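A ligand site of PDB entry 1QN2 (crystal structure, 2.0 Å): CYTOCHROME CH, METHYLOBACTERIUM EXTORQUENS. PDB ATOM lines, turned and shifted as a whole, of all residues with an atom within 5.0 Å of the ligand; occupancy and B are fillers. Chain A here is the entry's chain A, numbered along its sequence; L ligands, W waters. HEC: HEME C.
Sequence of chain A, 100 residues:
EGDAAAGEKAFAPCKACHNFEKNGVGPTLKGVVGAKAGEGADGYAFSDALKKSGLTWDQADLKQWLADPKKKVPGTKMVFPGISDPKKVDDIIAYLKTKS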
ATOM      1  N   PHE A  11      29.695  -6.987 -10.495  1.00  0.00           N
ATOM      2  CA  PHE A  11      28.970  -7.571  -9.393  1.00  0.00           C
ATOM      3  C   PHE A  11      29.071  -6.770  -8.121  1.00  0.00           C
ATOM      4  O   PHE A  11      28.377  -7.022  -7.121  1.00  0.00           O
ATOM      5  CB  PHE A  11      29.387  -9.023  -9.188  1.00  0.00           C
ATOM      6  CG  PHE A  11      28.569  -9.810  -8.213  1.00  0.00           C
ATOM      7  CD1 PHE A  11      27.395 -10.415  -8.590  1.00  0.00           C
ATOM      8  CD2 PHE A  11      29.009  -9.946  -6.902  1.00  0.00           C
ATOM      9  CE1 PHE A  11      26.621 -11.132  -7.706  1.00  0.00           C
ATOM     10  CE2 PHE A  11      28.251 -10.688  -6.024  1.00  0.00           C
ATOM     11  CZ  PHE A  11      27.061 -11.267  -6.395  1.00  0.00           C
ATOM     12  N   PRO A  13      27.918  -3.899  -6.878  1.00  0.00           N
ATOM     13  CA  PRO A  13      26.701  -3.474  -6.175  1.00  0.00           C
ATOM     14  C   PRO A  13      25.979  -4.625  -5.482  1.00  0.00           C
ATOM     15  O   PRO A  13      25.402  -4.430  -4.410  1.00  0.00           O
ATOM     16  CB  PRO A  13      25.826  -2.890  -7.286  1.00  0.00           C
ATOM     17  CG  PRO A  13      26.461  -3.301  -8.571  1.00  0.00           C
ATOM     18  CD  PRO A  13      27.941  -3.421  -8.265  1.00  0.00           C
ATOM     19  N   CYS A  14      25.994  -5.809  -6.077  1.00  0.00           N
ATOM     20  CA  CYS A  14      25.334  -6.976  -5.524  1.00  0.00           C
ATOM     21  C   CYS A  14      25.930  -7.477  -4.229  1.00  0.00           C
ATOM     22  O   CYS A  14      25.238  -8.112  -3.413  1.00  0.00           O
ATOM     23  CB  CYS A  14      25.339  -8.119  -6.569  1.00  0.00           C
ATOM     24  SG  CYS A  14      25.138  -7.525  -8.271  1.00  0.00           S
ATOM     25  N   ALA A  16      26.597  -6.055  -1.556  1.00  0.00           N
ATOM     26  CA  ALA A  16      25.940  -5.521  -0.376  1.00  0.00           C
ATOM     27  C   ALA A  16      24.951  -6.500   0.230  1.00  0.00           C
ATOM     28  O   ALA A  16      24.789  -6.546   1.451  1.00  0.00           O
ATOM     29  CB  ALA A  16      25.270  -4.189  -0.696  1.00  0.00           C
ATOM     30  N   CYS A  17      24.265  -7.282  -0.604  1.00  0.00           N
ATOM     31  CA  CYS A  17      23.286  -8.203  -0.050  1.00  0.00           C
ATOM     32  C   CYS A  17      23.515  -9.638  -0.489  1.00  0.00           C
ATOM     33  O   CYS A  17      22.764 -10.529  -0.067  1.00  0.00           O
ATOM     34  CB  CYS A  17      21.871  -7.770  -0.518  1.00  0.00           C
ATOM     35  SG  CYS A  17      21.596  -5.978  -0.443  1.00  0.00           S
ATOM     36  N   HIS A  18      24.520  -9.911  -1.318  1.00  0.00           N
ATOM     37  CA  HIS A  18      24.691 -11.306  -1.742  1.00  0.00           C
ATOM     38  C   HIS A  18      26.169 -11.722  -1.695  1.00  0.00           C
ATOM     39  O   HIS A  18      27.063 -10.919  -1.871  1.00  0.00           O
ATOM     40  CB  HIS A  18      24.254 -11.409  -3.228  1.00  0.00           C
ATOM     41  CG  HIS A  18      22.773 -11.296  -3.457  1.00  0.00           C
ATOM     42  ND1 HIS A  18      21.879 -12.249  -3.027  1.00  0.00           N
ATOM     43  CD2 HIS A  18      22.049 -10.351  -4.099  1.00  0.00           C
ATOM     44  CE1 HIS A  18      20.654 -11.895  -3.383  1.00  0.00           C
ATOM     45  NE2 HIS A  18      20.732 -10.748  -4.019  1.00  0.00           N
ATOM     46  N   VAL A  25      21.440 -10.226   3.942  1.00  0.00           N
ATOM     47  CA  VAL A  25      20.221  -9.436   3.642  1.00  0.00           C
ATOM     48  C   VAL A  25      19.478 -10.178   2.503  1.00  0.00           C
ATOM     49  O   VAL A  25      18.262 -10.281   2.510  1.00  0.00           O
ATOM     50  CB  VAL A  25      20.616  -8.045   3.098  1.00  0.00           C
ATOM     51  CG1 VAL A  25      19.428  -7.411   2.386  1.00  0.00           C
ATOM     52  CG2 VAL A  25      21.191  -7.159   4.177  1.00  0.00           C
ATOM     53  N   GLY A  26      20.281 -10.664   1.566  1.00  0.00           N
ATOM     54  CA  GLY A  26      19.807 -11.401   0.407  1.00  0.00           C
ATOM     55  C   GLY A  26      20.257 -12.849   0.480  1.00  0.00           C
ATOM     56  O   GLY A  26      21.130 -13.214   1.285  1.00  0.00           O
ATOM     57  N   PRO A  27      19.675 -13.718  -0.337  1.00  0.00           N
ATOM     58  CA  PRO A  27      20.057 -15.138  -0.241  1.00  0.00           C
ATOM     59  C   PRO A  27      21.408 -15.402  -0.913  1.00  0.00           C
ATOM     60  O   PRO A  27      21.898 -14.571  -1.673  1.00  0.00           O
ATOM     61  CB  PRO A  27      18.954 -15.823  -1.081  1.00  0.00           C
ATOM     62  CG  PRO A  27      18.710 -14.801  -2.167  1.00  0.00           C
ATOM     63  CD  PRO A  27      18.668 -13.496  -1.391  1.00  0.00           C
ATOM     64  N   LEU A  29      23.802 -16.818  -3.662  1.00  0.00           N
ATOM     65  CA  LEU A  29      23.566 -17.028  -5.094  1.00  0.00           C
ATOM     66  C   LEU A  29      24.254 -18.270  -5.605  1.00  0.00           C
ATOM     67  O   LEU A  29      24.361 -18.502  -6.813  1.00  0.00           O
ATOM     68  CB  LEU A  29      24.039 -15.793  -5.875  1.00  0.00           C
ATOM     69  CG  LEU A  29      23.222 -14.550  -5.525  1.00  0.00           C
ATOM     70  CD1 LEU A  29      23.572 -13.360  -6.387  1.00  0.00           C
ATOM     71  CD2 LEU A  29      21.726 -14.878  -5.558  1.00  0.00           C
ATOM     72  N   VAL A  32      22.602 -20.478  -8.484  1.00  0.00           N
ATOM     73  CA  VAL A  32      21.338 -19.828  -8.827  1.00  0.00           C
ATOM     74  C   VAL A  32      20.998 -19.938 -10.295  1.00  0.00           C
ATOM     75  O   VAL A  32      19.821 -19.924 -10.674  1.00  0.00           O
ATOM     76  CB  VAL A  32      21.320 -18.348  -8.392  1.00  0.00           C
ATOM     77  CG1 VAL A  32      22.278 -17.553  -9.274  1.00  0.00           C
ATOM     78  CG2 VAL A  32      19.879 -17.850  -8.495  1.00  0.00           C
ATOM     79  N   LYS A  36      15.180 -22.921  -9.668  1.00  0.00           N
ATOM     80  CA  LYS A  36      13.807 -22.365  -9.573  1.00  0.00           C
ATOM     81  C   LYS A  36      13.857 -21.161  -8.620  1.00  0.00           C
ATOM     82  O   LYS A  36      14.485 -21.263  -7.566  1.00  0.00           O
ATOM     83  CB  LYS A  36      12.892 -23.444  -8.980  1.00  0.00           C
ATOM     84  CG  LYS A  36      11.473 -23.421  -9.541  1.00  0.00           C
ATOM     85  CD  LYS A  36      10.578 -22.493  -8.735  1.00  0.00           C
ATOM     86  CE  LYS A  36       9.318 -23.190  -8.280  1.00  0.00           C
ATOM     87  NZ  LYS A  36       9.405 -23.670  -6.876  1.00  0.00           N
ATOM     88  N   ALA A  37      13.239 -20.041  -8.976  1.00  0.00           N
ATOM     89  CA  ALA A  37      13.276 -18.866  -8.136  1.00  0.00           C
ATOM     90  C   ALA A  37      12.503 -19.000  -6.845  1.00  0.00           C
ATOM     91  O   ALA A  37      11.460 -19.622  -6.764  1.00  0.00           O
ATOM     92  CB  ALA A  37      12.888 -17.619  -8.895  1.00  0.00           C
ATOM     93  N   GLY A  38      13.060 -18.388  -5.803  1.00  0.00           N
ATOM     94  CA  GLY A  38      12.524 -18.349  -4.475  1.00  0.00           C
ATOM     95  C   GLY A  38      12.241 -19.659  -3.781  1.00  0.00           C
ATOM     96  O   GLY A  38      11.362 -19.735  -2.929  1.00  0.00           O
ATOM     97  N   ALA A  41      18.388 -21.492  -1.664  1.00  0.00           N
ATOM     98  CA  ALA A  41      19.160 -20.620  -0.788  1.00  0.00           C
ATOM     99  C   ALA A  41      19.113 -21.075   0.659  1.00  0.00           C
ATOM    100  O   ALA A  41      18.882 -20.273   1.573  1.00  0.00           O
ATOM    101  CB  ALA A  41      18.715 -19.173  -0.931  1.00  0.00           C
ATOM    102  N   TYR A  44      16.217 -19.624   2.636  1.00  0.00           N
ATOM    103  CA  TYR A  44      16.137 -18.148   2.834  1.00  0.00           C
ATOM    104  C   TYR A  44      14.643 -17.777   2.827  1.00  0.00           C
ATOM    105  O   TYR A  44      13.884 -18.481   2.165  1.00  0.00           O
ATOM    106  CB  TYR A  44      16.838 -17.467   1.664  1.00  0.00           C
ATOM    107  CG  TYR A  44      16.717 -15.959   1.654  1.00  0.00           C
ATOM    108  CD1 TYR A  44      17.568 -15.161   2.410  1.00  0.00           C
ATOM    109  CD2 TYR A  44      15.688 -15.344   0.942  1.00  0.00           C
ATOM    110  CE1 TYR A  44      17.430 -13.786   2.417  1.00  0.00           C
ATOM    111  CE2 TYR A  44      15.555 -13.985   0.945  1.00  0.00           C
ATOM    112  CZ  TYR A  44      16.413 -13.210   1.684  1.00  0.00           C
ATOM    113  OH  TYR A  44      16.279 -11.843   1.697  1.00  0.00           O
ATOM    114  N   ALA A  45      14.246 -16.729   3.534  1.00  0.00           N
ATOM    115  CA  ALA A  45      12.850 -16.310   3.594  1.00  0.00           C
ATOM    116  C   ALA A  45      12.499 -15.400   2.417  1.00  0.00           C
ATOM    117  O   ALA A  45      12.589 -14.180   2.555  1.00  0.00           O
ATOM    118  CB  ALA A  45      12.589 -15.584   4.907  1.00  0.00           C
ATOM    119  N   PHE A  46      12.109 -15.982   1.297  1.00  0.00           N
ATOM    120  CA  PHE A  46      11.752 -15.201   0.118  1.00  0.00           C
ATOM    121  C   PHE A  46      10.369 -14.561   0.255  1.00  0.00           C
ATOM    122  O   PHE A  46       9.514 -15.002   1.018  1.00  0.00           O
ATOM    123  CB  PHE A  46      11.749 -16.108  -1.123  1.00  0.00           C
ATOM    124  CG  PHE A  46      13.124 -16.596  -1.508  1.00  0.00           C
ATOM    125  CD1 PHE A  46      13.989 -15.770  -2.212  1.00  0.00           C
ATOM    126  CD2 PHE A  46      13.509 -17.883  -1.201  1.00  0.00           C
ATOM    127  CE1 PHE A  46      15.232 -16.230  -2.602  1.00  0.00           C
ATOM    128  CE2 PHE A  46      14.759 -18.356  -1.579  1.00  0.00           C
ATOM    129  CZ  PHE A  46      15.622 -17.522  -2.271  1.00  0.00           C
ATOM    130  N   SER A  47      10.155 -13.502  -0.517  1.00  0.00           N
ATOM    131  CA  SER A  47       8.853 -12.813  -0.486  1.00  0.00           C
ATOM    132  C   SER A  47       7.802 -13.740  -1.111  1.00  0.00           C
ATOM    133  O   SER A  47       8.154 -14.686  -1.819  1.00  0.00           O
ATOM    134  CB  SER A  47       8.981 -11.563  -1.415  1.00  0.00           C
ATOM    135  OG  SER A  47       9.074 -12.014  -2.763  1.00  0.00           O
ATOM    136  N   LEU A  50       8.182 -13.585  -5.097  1.00  0.00           N
ATOM    137  CA  LEU A  50       9.185 -14.401  -5.813  1.00  0.00           C
ATOM    138  C   LEU A  50       8.880 -15.874  -5.711  1.00  0.00           C
ATOM    139  O   LEU A  50       8.939 -16.645  -6.689  1.00  0.00           O
ATOM    140  CB  LEU A  50      10.578 -14.101  -5.230  1.00  0.00           C
ATOM    141  CG  LEU A  50      11.699 -14.638  -6.148  1.00  0.00           C
ATOM    142  CD1 LEU A  50      11.519 -14.071  -7.559  1.00  0.00           C
ATOM    143  CD2 LEU A  50      13.057 -14.144  -5.627  1.00  0.00           C
ATOM    144  N   TRP A  57      15.435 -19.508 -13.226  1.00  0.00           N
ATOM    145  CA  TRP A  57      16.499 -18.592 -13.516  1.00  0.00           C
ATOM    146  C   TRP A  57      17.312 -18.903 -14.734  1.00  0.00           C
ATOM    147  O   TRP A  57      18.537 -19.095 -14.651  1.00  0.00           O
ATOM    148  CB  TRP A  57      17.362 -18.287 -12.307  1.00  0.00           C
ATOM    149  CG  TRP A  57      16.641 -17.488 -11.255  1.00  0.00           C
ATOM    150  CD1 TRP A  57      16.593 -17.737  -9.928  1.00  0.00           C
ATOM    151  CD2 TRP A  57      15.850 -16.308 -11.486  1.00  0.00           C
ATOM    152  NE1 TRP A  57      15.847 -16.761  -9.287  1.00  0.00           N
ATOM    153  CE2 TRP A  57      15.358 -15.901 -10.223  1.00  0.00           C
ATOM    154  CE3 TRP A  57      15.554 -15.546 -12.606  1.00  0.00           C
ATOM    155  CZ2 TRP A  57      14.577 -14.746 -10.069  1.00  0.00           C
ATOM    156  CZ3 TRP A  57      14.740 -14.430 -12.463  1.00  0.00           C
ATOM    157  CH2 TRP A  57      14.277 -14.043 -11.208  1.00  0.00           C
ATOM    158  N   LEU A  62      16.846 -14.162 -16.054  1.00  0.00           N
ATOM    159  CA  LEU A  62      17.814 -13.380 -15.269  1.00  0.00           C
ATOM    160  C   LEU A  62      18.055 -12.023 -15.916  1.00  0.00           C
ATOM    161  O   LEU A  62      18.259 -11.001 -15.276  1.00  0.00           O
ATOM    162  CB  LEU A  62      19.146 -14.151 -15.199  1.00  0.00           C
ATOM    163  CG  LEU A  62      19.210 -15.255 -14.139  1.00  0.00           C
ATOM    164  CD1 LEU A  62      20.529 -16.012 -14.179  1.00  0.00           C
ATOM    165  CD2 LEU A  62      18.956 -14.681 -12.746  1.00  0.00           C
ATOM    166  N   TRP A  65      15.139  -9.806 -14.979  1.00  0.00           N
ATOM    167  CA  TRP A  65      15.228  -9.607 -13.541  1.00  0.00           C
ATOM    168  C   TRP A  65      16.294  -8.603 -13.151  1.00  0.00           C
ATOM    169  O   TRP A  65      16.073  -7.717 -12.325  1.00  0.00           O
ATOM    170  CB  TRP A  65      15.474 -10.944 -12.842  1.00  0.00           C
ATOM    171  CG  TRP A  65      15.826 -10.918 -11.398  1.00  0.00           C
ATOM    172  CD1 TRP A  65      17.023 -11.255 -10.818  1.00  0.00           C
ATOM    173  CD2 TRP A  65      14.927 -10.612 -10.321  1.00  0.00           C
ATOM    174  NE1 TRP A  65      16.921 -11.161  -9.444  1.00  0.00           N
ATOM    175  CE2 TRP A  65      15.645 -10.759  -9.123  1.00  0.00           C
ATOM    176  CE3 TRP A  65      13.583 -10.230 -10.269  1.00  0.00           C
ATOM    177  CZ2 TRP A  65      15.068 -10.520  -7.879  1.00  0.00           C
ATOM    178  CZ3 TRP A  65      13.007  -9.999  -9.037  1.00  0.00           C
ATOM    179  CH2 TRP A  65      13.747 -10.152  -7.859  1.00  0.00           C
ATOM    180  N   LEU A  66      17.500  -8.705 -13.724  1.00  0.00           N
ATOM    181  CA  LEU A  66      18.542  -7.750 -13.362  1.00  0.00           C
ATOM    182  C   LEU A  66      18.299  -6.382 -13.959  1.00  0.00           C
ATOM    183  O   LEU A  66      18.705  -5.368 -13.366  1.00  0.00           O
ATOM    184  CB  LEU A  66      19.922  -8.288 -13.744  1.00  0.00           C
ATOM    185  CG  LEU A  66      20.351  -9.592 -13.062  1.00  0.00           C
ATOM    186  CD1 LEU A  66      21.844  -9.892 -13.305  1.00  0.00           C
ATOM    187  CD2 LEU A  66      20.115  -9.536 -11.553  1.00  0.00           C
ATOM    188  N   THR A  76       8.677  -7.981  -5.142  1.00  0.00           N
ATOM    189  CA  THR A  76       9.879  -8.632  -4.593  1.00  0.00           C
ATOM    190  C   THR A  76      10.503  -7.787  -3.494  1.00  0.00           C
ATOM    191  O   THR A  76      10.366  -6.556  -3.477  1.00  0.00           O
ATOM    192  CB  THR A  76      10.932  -8.815  -5.714  1.00  0.00           C
ATOM    193  OG1 THR A  76      12.155  -9.299  -5.109  1.00  0.00           O
ATOM    194  CG2 THR A  76      11.217  -7.482  -6.381  1.00  0.00           C
ATOM    195  N   LYS A  77      11.211  -8.417  -2.558  1.00  0.00           N
ATOM    196  CA  LYS A  77      11.833  -7.592  -1.516  1.00  0.00           C
ATOM    197  C   LYS A  77      13.246  -7.202  -1.914  1.00  0.00           C
ATOM    198  O   LYS A  77      14.009  -6.611  -1.140  1.00  0.00           O
ATOM    199  CB  LYS A  77      11.756  -8.200  -0.154  1.00  0.00           C
ATOM    200  CG  LYS A  77      12.391  -9.566   0.043  1.00  0.00           C
ATOM    201  CD  LYS A  77      12.225  -9.978   1.512  1.00  0.00           C
ATOM    202  CE  LYS A  77      12.518 -11.468   1.710  1.00  0.00           C
ATOM    203  NZ  LYS A  77      12.498 -11.803   3.169  1.00  0.00           N
ATOM    204  N   MET A  78      13.635  -7.525  -3.148  1.00  0.00           N
ATOM    205  CA  MET A  78      14.981  -7.114  -3.580  1.00  0.00           C
ATOM    206  C   MET A  78      14.933  -5.633  -4.004  1.00  0.00           C
ATOM    207  O   MET A  78      14.479  -5.341  -5.114  1.00  0.00           O
ATOM    208  CB  MET A  78      15.416  -7.947  -4.807  1.00  0.00           C
ATOM    209  CG  MET A  78      16.763  -7.415  -5.347  1.00  0.00           C
ATOM    210  SD  MET A  78      17.578  -8.703  -6.376  1.00  0.00           S
ATOM    211  CE  MET A  78      18.220  -7.587  -7.622  1.00  0.00           C
ATOM    212  N   VAL A  79      15.376  -4.771  -3.113  1.00  0.00           N
ATOM    213  CA  VAL A  79      15.390  -3.329  -3.366  1.00  0.00           C
ATOM    214  C   VAL A  79      16.674  -2.958  -4.133  1.00  0.00           C
ATOM    215  O   VAL A  79      17.725  -2.795  -3.530  1.00  0.00           O
ATOM    216  CB  VAL A  79      15.370  -2.533  -2.045  1.00  0.00           C
ATOM    217  CG1 VAL A  79      15.322  -1.041  -2.335  1.00  0.00           C
ATOM    218  CG2 VAL A  79      14.177  -2.977  -1.202  1.00  0.00           C
ATOM    219  N   PHE A  80      16.532  -2.885  -5.444  1.00  0.00           N
ATOM    220  CA  PHE A  80      17.634  -2.556  -6.373  1.00  0.00           C
ATOM    221  C   PHE A  80      17.017  -2.046  -7.678  1.00  0.00           C
ATOM    222  O   PHE A  80      16.145  -2.694  -8.238  1.00  0.00           O
ATOM    223  CB  PHE A  80      18.437  -3.832  -6.638  1.00  0.00           C
ATOM    224  CG  PHE A  80      19.646  -3.667  -7.510  1.00  0.00           C
ATOM    225  CD1 PHE A  80      20.727  -2.900  -7.099  1.00  0.00           C
ATOM    226  CD2 PHE A  80      19.704  -4.288  -8.744  1.00  0.00           C
ATOM    227  CE1 PHE A  80      21.832  -2.786  -7.920  1.00  0.00           C
ATOM    228  CE2 PHE A  80      20.803  -4.159  -9.577  1.00  0.00           C
ATOM    229  CZ  PHE A  80      21.883  -3.418  -9.129  1.00  0.00           C
ATOM    230  N   ILE A  83      20.040  -3.021 -13.571  1.00  0.00           N
ATOM    231  CA  ILE A  83      21.173  -2.605 -14.428  1.00  0.00           C
ATOM    232  C   ILE A  83      20.617  -2.293 -15.825  1.00  0.00           C
ATOM    233  O   ILE A  83      20.068  -3.176 -16.493  1.00  0.00           O
ATOM    234  CB  ILE A  83      22.184  -3.750 -14.540  1.00  0.00           C
ATOM    235  CG1 ILE A  83      22.584  -4.261 -13.158  1.00  0.00           C
ATOM    236  CG2 ILE A  83      23.405  -3.321 -15.332  1.00  0.00           C
ATOM    237  CD1 ILE A  83      23.829  -3.629 -12.587  1.00  0.00           C
ATOM    238  N   ILE A  92      27.438 -10.018 -15.910  1.00  0.00           N
ATOM    239  CA  ILE A  92      27.095 -10.513 -14.572  1.00  0.00           C
ATOM    240  C   ILE A  92      26.616 -11.951 -14.644  1.00  0.00           C
ATOM    241  O   ILE A  92      26.992 -12.796 -13.825  1.00  0.00           O
ATOM    242  CB  ILE A  92      26.014  -9.619 -13.934  1.00  0.00           C
ATOM    243  CG1 ILE A  92      26.600  -8.247 -13.601  1.00  0.00           C
ATOM    244  CG2 ILE A  92      25.437 -10.279 -12.692  1.00  0.00           C
ATOM    245  CD1 ILE A  92      25.730  -7.222 -12.962  1.00  0.00           C
ATOM    246  N   LEU A  96      27.954 -15.306 -12.705  1.00  0.00           N
ATOM    247  CA  LEU A  96      27.126 -16.162 -11.876  1.00  0.00           C
ATOM    248  C   LEU A  96      27.261 -17.626 -12.244  1.00  0.00           C
ATOM    249  O   LEU A  96      27.231 -18.509 -11.381  1.00  0.00           O
ATOM    250  CB  LEU A  96      25.651 -15.738 -11.981  1.00  0.00           C
ATOM    251  CG  LEU A  96      25.251 -14.372 -11.425  1.00  0.00           C
ATOM    252  CD1 LEU A  96      23.731 -14.189 -11.578  1.00  0.00           C
ATOM    253  CD2 LEU A  96      25.639 -14.270  -9.962  1.00  0.00           C
HETATM  254 FE   HEC L   1      19.463  -9.647  -5.209  1.00  0.00          FE
HETATM  255  CHA HEC L   1      17.086 -12.079  -4.792  1.00  0.00           C
HETATM  256  CHB HEC L   1      20.701 -11.327  -7.948  1.00  0.00           C
HETATM  257  CHC HEC L   1      21.387  -6.891  -6.040  1.00  0.00           C
HETATM  258  CHD HEC L   1      18.668  -8.257  -2.245  1.00  0.00           C
HETATM  259  NA  HEC L   1      18.996 -11.419  -6.186  1.00  0.00           N
HETATM  260  C1A HEC L   1      17.953 -12.257  -5.863  1.00  0.00           C
HETATM  261  C2A HEC L   1      17.940 -13.250  -6.800  1.00  0.00           C
HETATM  262  C3A HEC L   1      18.959 -13.048  -7.682  1.00  0.00           C
HETATM  263  C4A HEC L   1      19.611 -11.898  -7.306  1.00  0.00           C
HETATM  264  CMA HEC L   1      19.182 -14.020  -8.834  1.00  0.00           C
HETATM  265  CAA HEC L   1      16.981 -14.416  -6.860  1.00  0.00           C
HETATM  266  CBA HEC L   1      17.588 -15.598  -6.101  1.00  0.00           C
HETATM  267  CGA HEC L   1      16.650 -16.779  -5.889  1.00  0.00           C
HETATM  268  O1A HEC L   1      15.611 -16.930  -6.587  1.00  0.00           O
HETATM  269  O2A HEC L   1      17.122 -17.790  -5.313  1.00  0.00           O
HETATM  270  NB  HEC L   1      20.845  -9.198  -6.697  1.00  0.00           N
HETATM  271  C1B HEC L   1      21.214 -10.071  -7.681  1.00  0.00           C
HETATM  272  C2B HEC L   1      22.302  -9.513  -8.321  1.00  0.00           C
HETATM  273  C3B HEC L   1      22.449  -8.224  -7.863  1.00  0.00           C
HETATM  274  C4B HEC L   1      21.576  -8.053  -6.797  1.00  0.00           C
HETATM  275  CMB HEC L   1      23.131 -10.031  -9.481  1.00  0.00           C
HETATM  276  CAB HEC L   1      23.322  -7.287  -8.436  1.00  0.00           C
HETATM  277  CBB HEC L   1      23.100  -6.758  -9.699  1.00  0.00           C
HETATM  278  NC  HEC L   1      19.915  -7.843  -4.303  1.00  0.00           N
HETATM  279  C1C HEC L   1      20.779  -6.890  -4.783  1.00  0.00           C
HETATM  280  C2C HEC L   1      20.919  -5.968  -3.774  1.00  0.00           C
HETATM  281  C3C HEC L   1      20.179  -6.348  -2.684  1.00  0.00           C
HETATM  282  C4C HEC L   1      19.530  -7.518  -3.035  1.00  0.00           C
HETATM  283  CMC HEC L   1      21.736  -4.693  -3.629  1.00  0.00           C
HETATM  284  CAC HEC L   1      20.090  -5.673  -1.468  1.00  0.00           C
HETATM  285  CBC HEC L   1      19.775  -4.318  -1.364  1.00  0.00           C
HETATM  286  ND  HEC L   1      18.100 -10.116  -3.740  1.00  0.00           N
HETATM  287  C1D HEC L   1      17.925  -9.350  -2.631  1.00  0.00           C
HETATM  288  C2D HEC L   1      16.849  -9.884  -1.953  1.00  0.00           C
HETATM  289  C3D HEC L   1      16.424 -10.970  -2.656  1.00  0.00           C
HETATM  290  C4D HEC L   1      17.173 -11.120  -3.791  1.00  0.00           C
HETATM  291  CMD HEC L   1      16.162  -9.493  -0.661  1.00  0.00           C
HETATM  292  CAD HEC L   1      15.221 -11.837  -2.306  1.00  0.00           C
HETATM  293  CBD HEC L   1      14.117 -11.201  -3.168  1.00  0.00           C
HETATM  294  CGD HEC L   1      12.721 -11.681  -2.789  1.00  0.00           C
HETATM  295  O1D HEC L   1      11.755 -11.100  -3.360  1.00  0.00           O
HETATM  296  O2D HEC L   1      12.517 -12.645  -2.023  1.00  0.00           O
HETATM  297  O   HOH W   1      16.082 -20.363  -5.341  1.00  0.00           O
HETATM  298  O   HOH W   2      19.713 -18.328  -4.441  1.00  0.00           O
HETATM  299  O   HOH W   3      16.697  -5.753  -0.644  1.00  0.00           O
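A carbon (CAB) of the ligand is bonded to the side-chain sulfur (SG) of Cys 14 (1.8 Å).
SG of Cys 17 is bonded to CAC of the ligand (1.8 Å).
A ring nitrogen (NE2) of His 18 binds an iron atom (FE) of the ligand, 2.1 Å away.
FE of the ligand is bound by SD of Met 78, 2.4 Å away.
OG1 of Thr 76 lies within hydrogen-bond range of O1D of the ligand (2.5 Å).
The indole nitrogen (NE1) of Trp 57 sits at hydrogen-bond distance from an oxygen (O1A) of the ligand, at 2.7 Å.
The backbone NH (N) of Lys 77 lies within hydrogen-bond range of an oxygen (O1D) of the ligand, at 2.9 Å.
The backbone NH (N) of Ser 47 sits at hydrogen-bond distance from an oxygen (O2D) of the ligand.
The side-chain hydroxyl of Ser 47 lies within hydrogen-bond range of an oxygen (O1D) of the ligand, at 2.9 Å.
The backbone NH (N) of Gly 38 is in hydrogen-bond range of an oxygen (O1A) of the ligand.
The backbone NH (N) of Gly 26 is in hydrogen-bond range of the backbone carbonyl oxygen (O) of Cys 17, 3.0 Å away.
A ring nitrogen (ND1) of His 18 sits at hydrogen-bond distance from the backbone carbonyl oxygen (O) of Pro 27 (2.7 Å).
The side-chain hydroxyl of Thr 76 lies within hydrogen-bond range of the backbone NH of Met 78 (3.0 Å).
The side-chain amino group of Lys 77 lies within hydrogen-bond range of the backbone carbonyl oxygen of Ala 45.
The backbone NH of Leu 50 sits at hydrogen-bond distance from the side-chain hydroxyl of Ser 47 (3.0 Å).
The backbone carbonyl oxygen (O) of Val 25 sits at hydrogen-bond distance from the side-chain hydroxyl (OH) of Tyr 44, 2.7 Å away.
The backbone carbonyl oxygen of Leu 66 lies within hydrogen-bond range of the backbone NH of Ile 83 (2.7 Å).
Pro 13 touches the ligand.
Val 25 touches the ligand (O to CMD, 3.9 Å).
CD of Pro 27 touches C3D of the ligand (3.6 Å).
Leu 29 touches the ligand.
CG2 of Val 32 touches CMA of the ligand (3.9 Å).
Ala 37 touches the ligand (CA to O1A, 3.4 Å).
OH of Tyr 44 touches CMD of the ligand, at 3.3 Å.
Phe 46 touches the ligand (CZ to O2A, 3.4 Å).
Leu 50 touches the ligand.
Leu 62 touches the ligand (CD2 to CMA, 3.97 Å).
Trp 65 touches the ligand (NE1 to C3A, 3.3 Å).
CD2 of Leu 66 touches CMB of the ligand (3.7 Å).
Val 79 touches the ligand.
Phe 80 touches the ligand (CE2 to CBB, 3.5 Å).
Ile 92 touches the ligand.
Hydrophobic or aromatic side chains within 4 Å of the ligand: His 18, Pro 27, Leu 29, Val 32, Ala 37, Tyr 44, Phe 46, Leu 50, Trp 57, Leu 62, Trp 65, Leu 66, Met 78, Phe 80 and Ile 92.
24 residues have an atom within 4 Å of the ligand: Pro 13, Cys 14, Cys 17, His 18, Val 25, Pro 27, Leu 29, Val 32, Ala 37, Gly 38, Tyr 44, Phe 46, Ser 47, Leu 50, Trp 57, Leu 62, Trp 65, Leu 66, Thr 76, Lys 77, Met 78, Val 79, Phe 80 and Ile 92.
Water W1 lies within hydrogen-bond range of an oxygen (O2A) of the ligand (2.8 Å) and the backbone carbonyl oxygen of Lys 36 (2.9 Å).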
